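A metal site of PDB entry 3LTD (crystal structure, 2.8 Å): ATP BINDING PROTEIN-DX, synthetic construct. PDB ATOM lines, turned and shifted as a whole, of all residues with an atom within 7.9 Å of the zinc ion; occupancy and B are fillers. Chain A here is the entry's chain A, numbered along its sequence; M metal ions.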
ATOM      1  N   PRO A  24       9.480   7.232 -20.784  1.00  0.00           N
ATOM      2  CA  PRO A  24       9.516   7.198 -22.244  1.00  0.00           C
ATOM      3  C   PRO A  24      10.939   7.025 -22.777  1.00  0.00           C
ATOM      4  O   PRO A  24      11.887   7.037 -21.998  1.00  0.00           O
ATOM      5  CB  PRO A  24       8.978   8.590 -22.639  1.00  0.00           C
ATOM      6  CG  PRO A  24       9.378   9.461 -21.499  1.00  0.00           C
ATOM      7  CD  PRO A  24       9.299   8.597 -20.258  1.00  0.00           C
ATOM      8  N   CYS A  25      11.062   6.850 -24.092  1.00  0.00           N
ATOM      9  CA  CYS A  25      12.352   6.898 -24.775  1.00  0.00           C
ATOM     10  C   CYS A  25      13.320   7.904 -24.121  1.00  0.00           C
ATOM     11  O   CYS A  25      12.953   9.075 -23.944  1.00  0.00           O
ATOM     12  CB  CYS A  25      12.114   7.301 -26.218  1.00  0.00           C
ATOM     13  SG  CYS A  25      13.605   7.318 -27.218  1.00  0.00           S
ATOM     14  N   VAL A  26      14.542   7.489 -23.787  1.00  0.00           N
ATOM     15  CA  VAL A  26      15.536   8.439 -23.246  1.00  0.00           C
ATOM     16  C   VAL A  26      15.946   9.566 -24.222  1.00  0.00           C
ATOM     17  O   VAL A  26      16.330  10.636 -23.778  1.00  0.00           O
ATOM     18  CB  VAL A  26      16.819   7.759 -22.792  1.00  0.00           C
ATOM     19  CG1 VAL A  26      16.556   6.761 -21.660  1.00  0.00           C
ATOM     20  CG2 VAL A  26      17.458   7.062 -23.964  1.00  0.00           C
ATOM     21  N   LYS A  27      15.869   9.318 -25.526  1.00  0.00           N
ATOM     22  CA  LYS A  27      16.329  10.254 -26.568  1.00  0.00           C
ATOM     23  C   LYS A  27      15.268  11.301 -26.952  1.00  0.00           C
ATOM     24  O   LYS A  27      15.447  12.498 -26.724  1.00  0.00           O
ATOM     25  CB  LYS A  27      16.772   9.472 -27.831  1.00  0.00           C
ATOM     26  CG  LYS A  27      17.383  10.326 -28.930  1.00  0.00           C
ATOM     27  CD  LYS A  27      18.642  11.034 -28.439  1.00  0.00           C
ATOM     28  CE  LYS A  27      18.975  12.190 -29.357  1.00  0.00           C
ATOM     29  NZ  LYS A  27      20.370  12.661 -29.300  1.00  0.00           N
ATOM     30  N   CYS A  28      14.173  10.850 -27.566  1.00  0.00           N
ATOM     31  CA  CYS A  28      13.094  11.769 -27.927  1.00  0.00           C
ATOM     32  C   CYS A  28      12.188  12.080 -26.726  1.00  0.00           C
ATOM     33  O   CYS A  28      11.466  13.074 -26.730  1.00  0.00           O
ATOM     34  CB  CYS A  28      12.252  11.195 -29.079  1.00  0.00           C
ATOM     35  SG  CYS A  28      11.077   9.925 -28.519  1.00  0.00           S
ATOM     36  N   LYS A  29      12.215  11.241 -25.697  1.00  0.00           N
ATOM     37  CA  LYS A  29      11.411  11.595 -24.502  1.00  0.00           C
ATOM     38  C   LYS A  29       9.860  11.566 -24.667  1.00  0.00           C
ATOM     39  O   LYS A  29       9.156  11.993 -23.771  1.00  0.00           O
ATOM     40  CB  LYS A  29      11.798  13.003 -24.021  1.00  0.00           C
ATOM     41  CG  LYS A  29      13.054  13.031 -23.197  1.00  0.00           C
ATOM     42  CD  LYS A  29      14.006  14.151 -23.644  1.00  0.00           C
ATOM     43  CE  LYS A  29      15.176  14.246 -22.686  1.00  0.00           C
ATOM     44  NZ  LYS A  29      15.475  12.886 -22.151  1.00  0.00           N
ATOM     45  N   VAL A  30       9.356  11.073 -25.796  1.00  0.00           N
ATOM     46  CA  VAL A  30       7.911  10.999 -26.035  1.00  0.00           C
ATOM     47  C   VAL A  30       7.481   9.572 -26.408  1.00  0.00           C
ATOM     48  O   VAL A  30       6.701   8.947 -25.677  1.00  0.00           O
ATOM     49  CB  VAL A  30       7.490  11.996 -27.119  1.00  0.00           C
ATOM     50  CG1 VAL A  30       5.979  11.977 -27.290  1.00  0.00           C
ATOM     51  CG2 VAL A  30       7.966  13.371 -26.708  1.00  0.00           C
ATOM     52  N   ALA A  31       8.000   9.028 -27.513  1.00  0.00           N
ATOM     53  CA  ALA A  31       7.699   7.650 -27.845  1.00  0.00           C
ATOM     54  C   ALA A  31       7.979   6.730 -26.647  1.00  0.00           C
ATOM     55  O   ALA A  31       8.921   6.943 -25.860  1.00  0.00           O
ATOM     56  CB  ALA A  31       8.499   7.194 -29.058  1.00  0.00           C
ATOM     57  N   PRO A  32       7.147   5.692 -26.491  1.00  0.00           N
ATOM     58  CA  PRO A  32       7.496   4.624 -25.533  1.00  0.00           C
ATOM     59  C   PRO A  32       8.737   3.877 -26.017  1.00  0.00           C
ATOM     60  O   PRO A  32       9.147   4.017 -27.167  1.00  0.00           O
ATOM     61  CB  PRO A  32       6.269   3.688 -25.569  1.00  0.00           C
ATOM     62  CG  PRO A  32       5.211   4.412 -26.369  1.00  0.00           C
ATOM     63  CD  PRO A  32       5.906   5.406 -27.237  1.00  0.00           C
ATOM     64  N   ARG A  33       9.322   3.065 -25.154  1.00  0.00           N
ATOM     65  CA  ARG A  33      10.549   2.355 -25.510  1.00  0.00           C
ATOM     66  C   ARG A  33      10.319   1.069 -26.267  1.00  0.00           C
ATOM     67  O   ARG A  33       9.292   0.385 -26.106  1.00  0.00           O
ATOM     68  CB  ARG A  33      11.336   2.078 -24.243  1.00  0.00           C
ATOM     69  CG  ARG A  33      11.680   3.345 -23.489  1.00  0.00           C
ATOM     70  CD  ARG A  33      12.549   3.023 -22.303  1.00  0.00           C
ATOM     71  NE  ARG A  33      12.763   4.209 -21.480  1.00  0.00           N
ATOM     72  CZ  ARG A  33      13.604   4.254 -20.443  1.00  0.00           C
ATOM     73  NH1 ARG A  33      14.308   3.176 -20.095  1.00  0.00           N
ATOM     74  NH2 ARG A  33      13.732   5.374 -19.751  1.00  0.00           N
ATOM     75  N   ASP A  34      11.290   0.699 -27.086  1.00  0.00           N
ATOM     76  CA  ASP A  34      11.296  -0.648 -27.648  1.00  0.00           C
ATOM     77  C   ASP A  34      11.522  -1.631 -26.506  1.00  0.00           C
ATOM     78  O   ASP A  34      12.026  -1.263 -25.449  1.00  0.00           O
ATOM     79  CB  ASP A  34      12.379  -0.765 -28.714  1.00  0.00           C
ATOM     80  CG  ASP A  34      12.209  -2.022 -29.582  1.00  0.00           C
ATOM     81  OD1 ASP A  34      11.080  -2.550 -29.685  1.00  0.00           O
ATOM     82  OD2 ASP A  34      13.222  -2.469 -30.171  1.00  0.00           O
ATOM     83  N   ASN A  46      16.437   1.311 -23.917  1.00  0.00           N
ATOM     84  CA  ASN A  46      16.424   2.724 -23.552  1.00  0.00           C
ATOM     85  C   ASN A  46      15.689   3.651 -24.530  1.00  0.00           C
ATOM     86  O   ASN A  46      15.184   4.695 -24.121  1.00  0.00           O
ATOM     87  CB  ASN A  46      17.863   3.192 -23.289  1.00  0.00           C
ATOM     88  CG  ASN A  46      18.565   2.318 -22.260  1.00  0.00           C
ATOM     89  OD1 ASN A  46      17.956   1.887 -21.279  1.00  0.00           O
ATOM     90  ND2 ASN A  46      19.850   2.061 -22.476  1.00  0.00           N
ATOM     91  N   MET A  47      15.607   3.271 -25.812  1.00  0.00           N
ATOM     92  CA  MET A  47      14.950   4.108 -26.832  1.00  0.00           C
ATOM     93  C   MET A  47      13.763   3.458 -27.557  1.00  0.00           C
ATOM     94  O   MET A  47      13.603   2.237 -27.597  1.00  0.00           O
ATOM     95  CB  MET A  47      15.961   4.545 -27.879  1.00  0.00           C
ATOM     96  CG  MET A  47      17.113   5.358 -27.328  1.00  0.00           C
ATOM     97  SD  MET A  47      18.282   5.974 -28.584  1.00  0.00           S
ATOM     98  CE  MET A  47      19.469   4.644 -28.789  1.00  0.00           C
ATOM     99  N   CYS A  48      12.926   4.295 -28.155  1.00  0.00           N
ATOM    100  CA  CYS A  48      11.988   3.753 -29.133  1.00  0.00           C
ATOM    101  C   CYS A  48      12.781   3.241 -30.370  1.00  0.00           C
ATOM    102  O   CYS A  48      13.993   3.454 -30.493  1.00  0.00           O
ATOM    103  CB  CYS A  48      10.895   4.758 -29.505  1.00  0.00           C
ATOM    104  SG  CYS A  48      11.533   6.159 -30.328  1.00  0.00           S
ATOM    105  N   LYS A  49      12.114   2.526 -31.251  1.00  0.00           N
ATOM    106  CA  LYS A  49      12.792   2.010 -32.425  1.00  0.00           C
ATOM    107  C   LYS A  49      13.245   3.188 -33.303  1.00  0.00           C
ATOM    108  O   LYS A  49      14.362   3.166 -33.857  1.00  0.00           O
ATOM    109  CB  LYS A  49      11.855   1.131 -33.248  1.00  0.00           C
ATOM    110  CG  LYS A  49      12.588   0.179 -34.192  1.00  0.00           C
ATOM    111  CD  LYS A  49      13.217  -0.932 -33.383  1.00  0.00           C
ATOM    112  CE  LYS A  49      14.037  -1.847 -34.219  1.00  0.00           C
ATOM    113  NZ  LYS A  49      14.824  -2.641 -33.251  1.00  0.00           N
ATOM    114  N   THR A  50      12.377   4.200 -33.451  1.00  0.00           N
ATOM    115  CA  THR A  50      12.697   5.250 -34.386  1.00  0.00           C
ATOM    116  C   THR A  50      14.010   5.862 -33.965  1.00  0.00           C
ATOM    117  O   THR A  50      14.901   6.049 -34.804  1.00  0.00           O
ATOM    118  CB  THR A  50      11.635   6.319 -34.462  1.00  0.00           C
ATOM    119  OG1 THR A  50      10.467   5.764 -35.091  1.00  0.00           O
ATOM    120  CG2 THR A  50      12.154   7.513 -35.301  1.00  0.00           C
ATOM    121  N   CYS A  51      14.132   6.170 -32.675  1.00  0.00           N
ATOM    122  CA  CYS A  51      15.349   6.765 -32.185  1.00  0.00           C
ATOM    123  C   CYS A  51      16.534   5.825 -32.276  1.00  0.00           C
ATOM    124  O   CYS A  51      17.644   6.251 -32.607  1.00  0.00           O
ATOM    125  CB  CYS A  51      15.190   7.244 -30.757  1.00  0.00           C
ATOM    126  SG  CYS A  51      14.323   8.812 -30.685  1.00  0.00           S
ATOM    127  N   PHE A  52      16.311   4.555 -31.981  1.00  0.00           N
ATOM    128  CA  PHE A  52      17.416   3.609 -32.016  1.00  0.00           C
ATOM    129  C   PHE A  52      18.015   3.469 -33.409  1.00  0.00           C
ATOM    130  O   PHE A  52      19.255   3.534 -33.580  1.00  0.00           O
ATOM    131  CB  PHE A  52      16.977   2.259 -31.532  1.00  0.00           C
ATOM    132  CG  PHE A  52      18.032   1.227 -31.677  1.00  0.00           C
ATOM    133  CD1 PHE A  52      19.209   1.318 -30.925  1.00  0.00           C
ATOM    134  CD2 PHE A  52      17.888   0.184 -32.583  1.00  0.00           C
ATOM    135  CE1 PHE A  52      20.210   0.345 -31.054  1.00  0.00           C
ATOM    136  CE2 PHE A  52      18.894  -0.782 -32.734  1.00  0.00           C
ATOM    137  CZ  PHE A  52      20.053  -0.693 -31.958  1.00  0.00           C
HETATM  138 ZN    ZN M   1      12.613   8.036 -29.165  1.00  0.00          ZN
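The side-chain sulfur (SG) of Cys 28 sits close to the backbone NH (N) of Ala 31, 3.4 Å away.
The backbone NH of Val 30 lies close to the side-chain sulfur of Cys 28 (3.4 Å).
The backbone NH of Cys 25 lies within hydrogen-bond range of the backbone carbonyl oxygen of Ala 31, 2.8 Å away.
The side-chain sulfur (SG) of Cys 25 sits close to the backbone NH (N) of Lys 27.
The backbone NH of Thr 50 sits close to the side-chain sulfur of Cys 48 (3.8 Å).
Four residues have an atom within 4 Å of the zinc ion: Cys 25, Cys 28, Cys 48 and Cys 51.
The zinc ion is bound by the side-chain sulfur of Cys 25 (2.3 Å), the side-chain sulfur of Cys 51 (2.4 Å), the side-chain sulfur of Cys 48 (2.5 Å) and the side-chain sulfur of Cys 28 (2.5 Å).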
